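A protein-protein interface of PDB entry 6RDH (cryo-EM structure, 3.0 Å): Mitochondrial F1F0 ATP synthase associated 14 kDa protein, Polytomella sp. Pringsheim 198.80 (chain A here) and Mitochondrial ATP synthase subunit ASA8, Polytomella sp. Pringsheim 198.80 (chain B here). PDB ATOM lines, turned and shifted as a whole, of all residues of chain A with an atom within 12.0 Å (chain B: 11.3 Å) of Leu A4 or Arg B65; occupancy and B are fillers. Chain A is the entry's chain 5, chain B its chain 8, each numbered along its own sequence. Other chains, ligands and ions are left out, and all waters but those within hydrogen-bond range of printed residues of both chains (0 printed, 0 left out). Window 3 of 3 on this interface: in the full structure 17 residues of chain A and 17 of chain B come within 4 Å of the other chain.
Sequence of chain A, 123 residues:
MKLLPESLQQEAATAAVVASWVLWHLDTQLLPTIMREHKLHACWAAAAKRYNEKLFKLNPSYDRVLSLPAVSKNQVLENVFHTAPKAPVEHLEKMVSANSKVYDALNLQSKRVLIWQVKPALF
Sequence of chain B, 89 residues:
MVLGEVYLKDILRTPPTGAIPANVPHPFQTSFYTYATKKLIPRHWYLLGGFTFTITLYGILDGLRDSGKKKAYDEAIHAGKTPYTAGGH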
ATOM      1  N   MET A   1     -19.930 -23.953   5.125  1.00  0.00           N
ATOM      2  CA  MET A   1     -20.303 -23.557   3.773  1.00  0.00           C
ATOM      3  C   MET A   1     -19.083 -23.538   2.862  1.00  0.00           C
ATOM      4  O   MET A   1     -18.077 -24.187   3.139  1.00  0.00           O
ATOM      5  CB  MET A   1     -20.986 -22.186   3.786  1.00  0.00           C
ATOM      6  CG  MET A   1     -20.183 -21.098   4.479  1.00  0.00           C
ATOM      7  SD  MET A   1     -21.096 -19.572   4.744  1.00  0.00           S
ATOM      8  CE  MET A   1     -22.217 -20.074   6.044  1.00  0.00           C
ATOM      9  N   LYS A   2     -19.184 -22.798   1.765  1.00  0.00           N
ATOM     10  CA  LYS A   2     -18.050 -22.566   0.878  1.00  0.00           C
ATOM     11  C   LYS A   2     -17.241 -21.421   1.466  1.00  0.00           C
ATOM     12  O   LYS A   2     -17.537 -20.251   1.220  1.00  0.00           O
ATOM     13  CB  LYS A   2     -18.530 -22.246  -0.531  1.00  0.00           C
ATOM     14  CG  LYS A   2     -17.427 -22.088  -1.558  1.00  0.00           C
ATOM     15  CD  LYS A   2     -16.706 -23.403  -1.797  1.00  0.00           C
ATOM     16  CE  LYS A   2     -15.681 -23.285  -2.912  1.00  0.00           C
ATOM     17  NZ  LYS A   2     -16.325 -23.109  -4.240  1.00  0.00           N
ATOM     18  N   LEU A   3     -16.216 -21.750   2.245  1.00  0.00           N
ATOM     19  CA  LEU A   3     -15.335 -20.736   2.804  1.00  0.00           C
ATOM     20  C   LEU A   3     -13.953 -20.797   2.177  1.00  0.00           C
ATOM     21  O   LEU A   3     -13.493 -19.801   1.618  1.00  0.00           O
ATOM     22  CB  LEU A   3     -15.228 -20.880   4.323  1.00  0.00           C
ATOM     23  CG  LEU A   3     -16.407 -20.431   5.178  1.00  0.00           C
ATOM     24  CD1 LEU A   3     -15.927 -20.255   6.588  1.00  0.00           C
ATOM     25  CD2 LEU A   3     -17.004 -19.147   4.668  1.00  0.00           C
ATOM     26  N   LEU A   4     -13.285 -21.937   2.247  1.00  0.00           N
ATOM     27  CA  LEU A   4     -12.081 -21.936   1.435  1.00  0.00           C
ATOM     28  C   LEU A   4     -12.385 -22.527   0.067  1.00  0.00           C
ATOM     29  O   LEU A   4     -13.172 -23.467  -0.037  1.00  0.00           O
ATOM     30  CB  LEU A   4     -10.967 -22.726   2.103  1.00  0.00           C
ATOM     31  CG  LEU A   4     -10.035 -21.876   2.959  1.00  0.00           C
ATOM     32  CD1 LEU A   4     -10.614 -21.651   4.333  1.00  0.00           C
ATOM     33  CD2 LEU A   4      -8.678 -22.500   3.058  1.00  0.00           C
ATOM     34  N   PRO A   5     -11.815 -21.998  -1.001  1.00  0.00           N
ATOM     35  CA  PRO A   5     -12.053 -22.559  -2.329  1.00  0.00           C
ATOM     36  C   PRO A   5     -11.263 -23.849  -2.497  1.00  0.00           C
ATOM     37  O   PRO A   5     -10.441 -24.209  -1.661  1.00  0.00           O
ATOM     38  CB  PRO A   5     -11.550 -21.462  -3.258  1.00  0.00           C
ATOM     39  CG  PRO A   5     -10.506 -20.802  -2.486  1.00  0.00           C
ATOM     40  CD  PRO A   5     -10.949 -20.815  -1.065  1.00  0.00           C
ATOM     41  N   GLU A   6     -11.526 -24.545  -3.602  1.00  0.00           N
ATOM     42  CA  GLU A   6     -10.831 -25.800  -3.835  1.00  0.00           C
ATOM     43  C   GLU A   6      -9.366 -25.565  -4.175  1.00  0.00           C
ATOM     44  O   GLU A   6      -8.515 -26.404  -3.864  1.00  0.00           O
ATOM     45  CB  GLU A   6     -11.526 -26.593  -4.938  1.00  0.00           C
ATOM     46  CG  GLU A   6     -13.037 -26.818  -4.737  1.00  0.00           C
ATOM     47  CD  GLU A   6     -13.426 -27.574  -3.462  1.00  0.00           C
ATOM     48  OE1 GLU A   6     -12.614 -28.337  -2.902  1.00  0.00           O
ATOM     49  OE2 GLU A   6     -14.587 -27.432  -3.031  1.00  0.00           O
ATOM     50  N   SER A   7      -9.056 -24.437  -4.805  1.00  0.00           N
ATOM     51  CA  SER A   7      -7.683 -23.987  -4.986  1.00  0.00           C
ATOM     52  C   SER A   7      -7.643 -22.484  -4.786  1.00  0.00           C
ATOM     53  O   SER A   7      -8.342 -21.750  -5.484  1.00  0.00           O
ATOM     54  CB  SER A   7      -7.150 -24.348  -6.367  1.00  0.00           C
ATOM     55  OG  SER A   7      -5.754 -24.132  -6.426  1.00  0.00           O
ATOM     56  N   LEU A   8      -6.833 -22.030  -3.834  1.00  0.00           N
ATOM     57  CA  LEU A   8      -6.730 -20.601  -3.573  1.00  0.00           C
ATOM     58  C   LEU A   8      -5.951 -19.890  -4.661  1.00  0.00           C
ATOM     59  O   LEU A   8      -6.242 -18.732  -4.977  1.00  0.00           O
ATOM     60  CB  LEU A   8      -6.062 -20.365  -2.226  1.00  0.00           C
ATOM     61  CG  LEU A   8      -6.934 -20.377  -0.982  1.00  0.00           C
ATOM     62  CD1 LEU A   8      -6.066 -20.591   0.216  1.00  0.00           C
ATOM     63  CD2 LEU A   8      -7.667 -19.078  -0.860  1.00  0.00           C
ATOM     64  N   GLN A   9      -4.954 -20.561  -5.237  1.00  0.00           N
ATOM     65  CA  GLN A   9      -4.133 -19.949  -6.273  1.00  0.00           C
ATOM     66  C   GLN A   9      -4.903 -19.774  -7.565  1.00  0.00           C
ATOM     67  O   GLN A   9      -4.665 -18.811  -8.291  1.00  0.00           O
ATOM     68  CB  GLN A   9      -2.893 -20.791  -6.525  1.00  0.00           C
ATOM     69  CG  GLN A   9      -1.839 -20.110  -7.336  1.00  0.00           C
ATOM     70  CD  GLN A   9      -0.743 -21.049  -7.727  1.00  0.00           C
ATOM     71  OE1 GLN A   9      -0.973 -22.238  -7.902  1.00  0.00           O
ATOM     72  NE2 GLN A   9       0.462 -20.529  -7.863  1.00  0.00           N
ATOM     73  N   GLN A  10      -5.834 -20.679  -7.859  1.00  0.00           N
ATOM     74  CA  GLN A  10      -6.669 -20.527  -9.042  1.00  0.00           C
ATOM     75  C   GLN A  10      -7.579 -19.317  -8.924  1.00  0.00           C
ATOM     76  O   GLN A  10      -7.747 -18.565  -9.886  1.00  0.00           O
ATOM     77  CB  GLN A  10      -7.497 -21.783  -9.256  1.00  0.00           C
ATOM     78  CG  GLN A  10      -8.489 -21.674 -10.374  1.00  0.00           C
ATOM     79  CD  GLN A  10      -9.368 -22.874 -10.459  1.00  0.00           C
ATOM     80  OE1 GLN A  10     -10.317 -23.016  -9.696  1.00  0.00           O
ATOM     81  NE2 GLN A  10      -9.048 -23.770 -11.374  1.00  0.00           N
ATOM     82  N   GLU A  11      -8.147 -19.091  -7.742  1.00  0.00           N
ATOM     83  CA  GLU A  11      -9.003 -17.930  -7.550  1.00  0.00           C
ATOM     84  C   GLU A  11      -8.204 -16.637  -7.533  1.00  0.00           C
ATOM     85  O   GLU A  11      -8.655 -15.620  -8.070  1.00  0.00           O
ATOM     86  CB  GLU A  11      -9.802 -18.085  -6.270  1.00  0.00           C
ATOM     87  CG  GLU A  11     -11.099 -18.808  -6.467  1.00  0.00           C
ATOM     88  CD  GLU A  11     -12.059 -18.563  -5.329  1.00  0.00           C
ATOM     89  OE1 GLU A  11     -11.596 -18.190  -4.240  1.00  0.00           O
ATOM     90  OE2 GLU A  11     -13.278 -18.725  -5.524  1.00  0.00           O
ATOM     91  N   ALA A  12      -7.009 -16.653  -6.939  1.00  0.00           N
ATOM     92  CA  ALA A  12      -6.159 -15.470  -6.991  1.00  0.00           C
ATOM     93  C   ALA A  12      -5.676 -15.184  -8.403  1.00  0.00           C
ATOM     94  O   ALA A  12      -5.564 -14.020  -8.796  1.00  0.00           O
ATOM     95  CB  ALA A  12      -4.971 -15.629  -6.056  1.00  0.00           C
ATOM     96  N   ALA A  13      -5.434 -16.224  -9.199  1.00  0.00           N
ATOM     97  CA  ALA A  13      -5.042 -16.020 -10.584  1.00  0.00           C
ATOM     98  C   ALA A  13      -6.213 -15.572 -11.435  1.00  0.00           C
ATOM     99  O   ALA A  13      -6.014 -14.842 -12.400  1.00  0.00           O
ATOM    100  CB  ALA A  13      -4.431 -17.291 -11.153  1.00  0.00           C
ATOM    101  N   THR B  56       1.962 -16.389  -6.239  1.00  0.00           N
ATOM    102  CA  THR B  56       2.945 -17.259  -5.593  1.00  0.00           C
ATOM    103  C   THR B  56       2.618 -17.498  -4.124  1.00  0.00           C
ATOM    104  O   THR B  56       2.796 -18.614  -3.628  1.00  0.00           O
ATOM    105  CB  THR B  56       4.348 -16.689  -5.724  1.00  0.00           C
ATOM    106  OG1 THR B  56       4.390 -15.387  -5.143  1.00  0.00           O
ATOM    107  CG2 THR B  56       4.755 -16.620  -7.174  1.00  0.00           C
ATOM    108  N   LEU B  57       2.116 -16.482  -3.419  1.00  0.00           N
ATOM    109  CA  LEU B  57       1.754 -16.655  -2.016  1.00  0.00           C
ATOM    110  C   LEU B  57       0.579 -17.606  -1.857  1.00  0.00           C
ATOM    111  O   LEU B  57       0.547 -18.421  -0.929  1.00  0.00           O
ATOM    112  CB  LEU B  57       1.424 -15.302  -1.399  1.00  0.00           C
ATOM    113  CG  LEU B  57       0.978 -15.324   0.056  1.00  0.00           C
ATOM    114  CD1 LEU B  57       2.161 -15.620   0.946  1.00  0.00           C
ATOM    115  CD2 LEU B  57       0.322 -14.023   0.433  1.00  0.00           C
ATOM    116  N   TYR B  58      -0.377 -17.553  -2.768  1.00  0.00           N
ATOM    117  CA  TYR B  58      -1.505 -18.455  -2.645  1.00  0.00           C
ATOM    118  C   TYR B  58      -1.160 -19.844  -3.141  1.00  0.00           C
ATOM    119  O   TYR B  58      -1.771 -20.814  -2.692  1.00  0.00           O
ATOM    120  CB  TYR B  58      -2.713 -17.887  -3.378  1.00  0.00           C
ATOM    121  CG  TYR B  58      -3.471 -16.858  -2.573  1.00  0.00           C
ATOM    122  CD1 TYR B  58      -2.847 -15.725  -2.094  1.00  0.00           C
ATOM    123  CD2 TYR B  58      -4.808 -17.016  -2.300  1.00  0.00           C
ATOM    124  CE1 TYR B  58      -3.513 -14.802  -1.373  1.00  0.00           C
ATOM    125  CE2 TYR B  58      -5.487 -16.086  -1.570  1.00  0.00           C
ATOM    126  CZ  TYR B  58      -4.827 -14.986  -1.117  1.00  0.00           C
ATOM    127  OH  TYR B  58      -5.485 -14.046  -0.394  1.00  0.00           O
ATOM    128  N   GLY B  59      -0.151 -19.968  -4.005  1.00  0.00           N
ATOM    129  CA  GLY B  59       0.408 -21.279  -4.280  1.00  0.00           C
ATOM    130  C   GLY B  59       1.100 -21.870  -3.071  1.00  0.00           C
ATOM    131  O   GLY B  59       1.008 -23.075  -2.825  1.00  0.00           O
ATOM    132  N   ILE B  60       1.781 -21.027  -2.289  1.00  0.00           N
ATOM    133  CA  ILE B  60       2.387 -21.462  -1.029  1.00  0.00           C
ATOM    134  C   ILE B  60       1.316 -21.947  -0.055  1.00  0.00           C
ATOM    135  O   ILE B  60       1.459 -23.005   0.568  1.00  0.00           O
ATOM    136  CB  ILE B  60       3.230 -20.324  -0.420  1.00  0.00           C
ATOM    137  CG1 ILE B  60       4.465 -20.032  -1.259  1.00  0.00           C
ATOM    138  CG2 ILE B  60       3.659 -20.648   0.979  1.00  0.00           C
ATOM    139  CD1 ILE B  60       5.297 -21.217  -1.537  1.00  0.00           C
ATOM    140  N   LEU B  61       0.216 -21.202   0.061  1.00  0.00           N
ATOM    141  CA  LEU B  61      -0.858 -21.597   0.971  1.00  0.00           C
ATOM    142  C   LEU B  61      -1.574 -22.858   0.496  1.00  0.00           C
ATOM    143  O   LEU B  61      -2.002 -23.680   1.315  1.00  0.00           O
ATOM    144  CB  LEU B  61      -1.859 -20.461   1.135  1.00  0.00           C
ATOM    145  CG  LEU B  61      -1.362 -19.158   1.745  1.00  0.00           C
ATOM    146  CD1 LEU B  61      -2.532 -18.241   2.022  1.00  0.00           C
ATOM    147  CD2 LEU B  61      -0.575 -19.423   3.000  1.00  0.00           C
ATOM    148  N   ASP B  62      -1.704 -23.043  -0.819  1.00  0.00           N
ATOM    149  CA  ASP B  62      -2.268 -24.287  -1.334  1.00  0.00           C
ATOM    150  C   ASP B  62      -1.343 -25.468  -1.075  1.00  0.00           C
ATOM    151  O   ASP B  62      -1.810 -26.584  -0.818  1.00  0.00           O
ATOM    152  CB  ASP B  62      -2.544 -24.154  -2.828  1.00  0.00           C
ATOM    153  CG  ASP B  62      -3.886 -23.537  -3.117  1.00  0.00           C
ATOM    154  OD1 ASP B  62      -4.771 -23.598  -2.242  1.00  0.00           O
ATOM    155  OD2 ASP B  62      -4.061 -23.004  -4.231  1.00  0.00           O
ATOM    156  N   GLY B  63      -0.031 -25.238  -1.139  1.00  0.00           N
ATOM    157  CA  GLY B  63       0.911 -26.288  -0.794  1.00  0.00           C
ATOM    158  C   GLY B  63       0.849 -26.662   0.672  1.00  0.00           C
ATOM    159  O   GLY B  63       0.919 -27.844   1.019  1.00  0.00           O
ATOM    160  N   LEU B  64       0.675 -25.665   1.544  1.00  0.00           N
ATOM    161  CA  LEU B  64       0.500 -25.943   2.969  1.00  0.00           C
ATOM    162  C   LEU B  64      -0.780 -26.723   3.223  1.00  0.00           C
ATOM    163  O   LEU B  64      -0.793 -27.661   4.029  1.00  0.00           O
ATOM    164  CB  LEU B  64       0.480 -24.650   3.776  1.00  0.00           C
ATOM    165  CG  LEU B  64       1.715 -23.759   3.787  1.00  0.00           C
ATOM    166  CD1 LEU B  64       1.551 -22.696   4.836  1.00  0.00           C
ATOM    167  CD2 LEU B  64       2.967 -24.554   4.020  1.00  0.00           C
ATOM    168  N   ARG B  65      -1.851 -26.386   2.506  1.00  0.00           N
ATOM    169  CA  ARG B  65      -3.120 -27.063   2.737  1.00  0.00           C
ATOM    170  C   ARG B  65      -3.101 -28.502   2.238  1.00  0.00           C
ATOM    171  O   ARG B  65      -3.604 -29.401   2.923  1.00  0.00           O
ATOM    172  CB  ARG B  65      -4.253 -26.295   2.079  1.00  0.00           C
ATOM    173  CG  ARG B  65      -5.602 -26.745   2.541  1.00  0.00           C
ATOM    174  CD  ARG B  65      -6.535 -25.574   2.648  1.00  0.00           C
ATOM    175  NE  ARG B  65      -6.553 -24.806   1.415  1.00  0.00           N
ATOM    176  CZ  ARG B  65      -7.454 -24.974   0.459  1.00  0.00           C
ATOM    177  NH1 ARG B  65      -7.399 -24.237  -0.635  1.00  0.00           N
ATOM    178  NH2 ARG B  65      -8.409 -25.878   0.602  1.00  0.00           N
ATOM    179  N   ASP B  66      -2.518 -28.760   1.063  1.00  0.00           N
ATOM    180  CA  ASP B  66      -2.505 -30.151   0.621  1.00  0.00           C
ATOM    181  C   ASP B  66      -1.465 -30.976   1.374  1.00  0.00           C
ATOM    182  O   ASP B  66      -1.644 -32.186   1.515  1.00  0.00           O
ATOM    183  CB  ASP B  66      -2.372 -30.277  -0.910  1.00  0.00           C
ATOM    184  CG  ASP B  66      -1.099 -29.673  -1.492  1.00  0.00           C
ATOM    185  OD1 ASP B  66      -1.186 -29.174  -2.633  1.00  0.00           O
ATOM    186  OD2 ASP B  66      -0.008 -29.736  -0.895  1.00  0.00           O
ATOM    187  N   SER B  67      -0.398 -30.358   1.898  1.00  0.00           N
ATOM    188  CA  SER B  67       0.491 -31.120   2.772  1.00  0.00           C
ATOM    189  C   SER B  67      -0.172 -31.444   4.105  1.00  0.00           C
ATOM    190  O   SER B  67       0.082 -32.509   4.675  1.00  0.00           O
ATOM    191  CB  SER B  67       1.797 -30.371   3.007  1.00  0.00           C
ATOM    192  OG  SER B  67       1.582 -29.227   3.798  1.00  0.00           O
ATOM    193  N   GLY B  68      -1.039 -30.563   4.604  1.00  0.00           N
ATOM    194  CA  GLY B  68      -1.816 -30.903   5.786  1.00  0.00           C
ATOM    195  C   GLY B  68      -2.814 -32.018   5.530  1.00  0.00           C
ATOM    196  O   GLY B  68      -3.008 -32.897   6.378  1.00  0.00           O
ATOM    197  N   LYS B  69      -3.452 -31.999   4.355  1.00  0.00           N
ATOM    198  CA  LYS B  69      -4.329 -33.099   3.954  1.00  0.00           C
ATOM    199  C   LYS B  69      -3.558 -34.405   3.827  1.00  0.00           C
ATOM    200  O   LYS B  69      -4.062 -35.467   4.207  1.00  0.00           O
ATOM    201  CB  LYS B  69      -5.002 -32.783   2.623  1.00  0.00           C
ATOM    202  CG  LYS B  69      -6.161 -31.830   2.668  1.00  0.00           C
ATOM    203  CD  LYS B  69      -6.724 -31.698   1.276  1.00  0.00           C
ATOM    204  CE  LYS B  69      -7.896 -30.760   1.225  1.00  0.00           C
ATOM    205  NZ  LYS B  69      -8.483 -30.737  -0.139  1.00  0.00           N
ATOM    206  N   LYS B  70      -2.334 -34.341   3.297  1.00  0.00           N
ATOM    207  CA  LYS B  70      -1.498 -35.528   3.161  1.00  0.00           C
ATOM    208  C   LYS B  70      -1.102 -36.080   4.516  1.00  0.00           C
ATOM    209  O   LYS B  70      -1.101 -37.298   4.714  1.00  0.00           O
ATOM    210  CB  LYS B  70      -0.250 -35.198   2.348  1.00  0.00           C
ATOM    211  CG  LYS B  70       0.662 -36.373   2.102  1.00  0.00           C
ATOM    212  CD  LYS B  70       1.860 -35.970   1.273  1.00  0.00           C
ATOM    213  CE  LYS B  70       2.688 -37.178   0.866  1.00  0.00           C
ATOM    214  NZ  LYS B  70       3.285 -37.873   2.032  1.00  0.00           N
ATOM    215  N   LYS B  71      -0.784 -35.197   5.464  1.00  0.00           N
ATOM    216  CA  LYS B  71      -0.427 -35.628   6.812  1.00  0.00           C
ATOM    217  C   LYS B  71      -1.601 -36.308   7.506  1.00  0.00           C
ATOM    218  O   LYS B  71      -1.440 -37.375   8.112  1.00  0.00           O
ATOM    219  CB  LYS B  71       0.063 -34.430   7.618  1.00  0.00           C
ATOM    220  CG  LYS B  71      -0.007 -34.607   9.109  1.00  0.00           C
ATOM    221  CD  LYS B  71       0.260 -33.311   9.828  1.00  0.00           C
ATOM    222  CE  LYS B  71       0.284 -33.534  11.319  1.00  0.00           C
ATOM    223  NZ  LYS B  71       1.325 -34.528  11.675  1.00  0.00           N
ATOM    224  N   ALA B  72      -2.797 -35.724   7.397  1.00  0.00           N
ATOM    225  CA  ALA B  72      -3.972 -36.328   8.024  1.00  0.00           C
ATOM    226  C   ALA B  72      -4.341 -37.657   7.372  1.00  0.00           C
ATOM    227  O   ALA B  72      -4.694 -38.616   8.069  1.00  0.00           O
ATOM    228  CB  ALA B  72      -5.152 -35.362   7.973  1.00  0.00           C
ATOM    229  N   TYR B  73      -4.226 -37.743   6.043  1.00  0.00           N
ATOM    230  CA  TYR B  73      -4.513 -38.984   5.331  1.00  0.00           C
ATOM    231  C   TYR B  73      -3.506 -40.072   5.681  1.00  0.00           C
ATOM    232  O   TYR B  73      -3.874 -41.241   5.842  1.00  0.00           O
ATOM    233  CB  TYR B  73      -4.509 -38.714   3.831  1.00  0.00           C
ATOM    234  CG  TYR B  73      -5.182 -39.751   2.974  1.00  0.00           C
ATOM    235  CD1 TYR B  73      -6.555 -39.767   2.827  1.00  0.00           C
ATOM    236  CD2 TYR B  73      -4.438 -40.681   2.271  1.00  0.00           C
ATOM    237  CE1 TYR B  73      -7.176 -40.698   2.039  1.00  0.00           C
ATOM    238  CE2 TYR B  73      -5.048 -41.616   1.472  1.00  0.00           C
ATOM    239  CZ  TYR B  73      -6.418 -41.619   1.358  1.00  0.00           C
ATOM    240  OH  TYR B  73      -7.033 -42.553   0.560  1.00  0.00           O
ATOM    241  N   ASP B  74      -2.232 -39.701   5.831  1.00  0.00           N
ATOM    242  CA  ASP B  74      -1.210 -40.674   6.194  1.00  0.00           C
ATOM    243  C   ASP B  74      -1.395 -41.174   7.618  1.00  0.00           C
ATOM    244  O   ASP B  74      -1.207 -42.363   7.886  1.00  0.00           O
ATOM    245  CB  ASP B  74       0.179 -40.065   6.031  1.00  0.00           C
ATOM    246  CG  ASP B  74       0.607 -39.985   4.594  1.00  0.00           C
ATOM    247  OD1 ASP B  74      -0.186 -40.376   3.716  1.00  0.00           O
ATOM    248  OD2 ASP B  74       1.739 -39.532   4.337  1.00  0.00           O
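Arg B65 touches Leu A4 (NE to CD2, 3.5 Å). O of Leu A8 touches CD2 of Tyr B58, 3.5 Å away. Leu A8 touches Arg B65 (CG to NH1, 3.9 Å). Tyr B58 touches Gln A9 (CB to CA, 3.8 Å). Gly B59 touches Gln A9. Tyr B58 touches Ala A12.
Printed residues of chain A that touch a printed residue of chain B: Leu A4, Pro A5, Ser A7, Leu A8, Gln A9 and Ala A12. Hydrophobic or aromatic side chains of chain A that line the printed part of chain B: Leu A4, Leu A8 and Ala A12. Along chain A the printed residues that touch a printed residue of chain B span positions 4 to 12. Among the printed residues, no Asp or Glu carboxylate lies within 4 Å of a Lys or Arg side-chain nitrogen of the other chain.
Of chain B, only Arg B65 (3.5 Å) comes within 4 Å of Leu A4. Of the printed residues of chain A, Arg B65 touches Leu A4, Pro A5 and Leu A8. No residue of chain B comes within 4 Å of Leu A3. No residue of chain B comes within 4 Å of Glu A6. Ser A7 touches just one residue of chain B: Asp B62 (3.0 Å). No residue of chain A comes within 4 Å of Leu B61. Asp B62 touches just these residues of chain A: Ser A7, Leu A8 and Gln A9. No residue of chain A comes within 4 Å of Gly B63. No residue of chain A comes within 4 Å of Leu B64. No residue of chain A comes within 4 Å of Asp B66. No residue of chain A comes within 4 Å of Ser B67. No residue of chain A comes within 4 Å of Gly B68. Printed residues of chain B within 4 Å of Gln A9: Tyr B58 (3.8 Å), Gly B59 (3.6 Å) and Asp B62 (2.8 Å). Of the printed residues of chain A, Tyr B58 touches Leu A8, Gln A9 and Ala A12. Of the printed residues of chain A, Gly B59 touches Gln A9. Of the printed residues of chain B, Ala A12 touches Tyr B58 (3.99 Å). Tyr B73 touches none of the printed residues of chain A. Lys B71 touches none of the printed residues of chain A. The nearest residue of chain B that does not touch Leu A4 is Asp B62 (6.7 Å). The nearest printed residue of chain A that does not touch Tyr B58 is Gln A10 (6.1 Å).
The side-chain carboxylate of Asp B62 is in salt-bridge range of the guanidinium group of Arg B65, 3.1 Å away.
The guanidinium group of Arg B65 sits at hydrogen-bond distance from the backbone carbonyl oxygen of Pro A5, at 3.2 Å. The backbone NH (N) of Gln A9 is in hydrogen-bond range of the side-chain carboxylate (OD2) of Asp B62 (2.8 Å). The side-chain carboxylate (OD2) of Asp B62 sits at hydrogen-bond distance from the backbone NH (N) of Leu A8 (3.0 Å). The side-chain hydroxyl (OG) of Ser A7 is in hydrogen-bond range of the side-chain carboxylate (OD2) of Asp B62 (3.0 Å).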
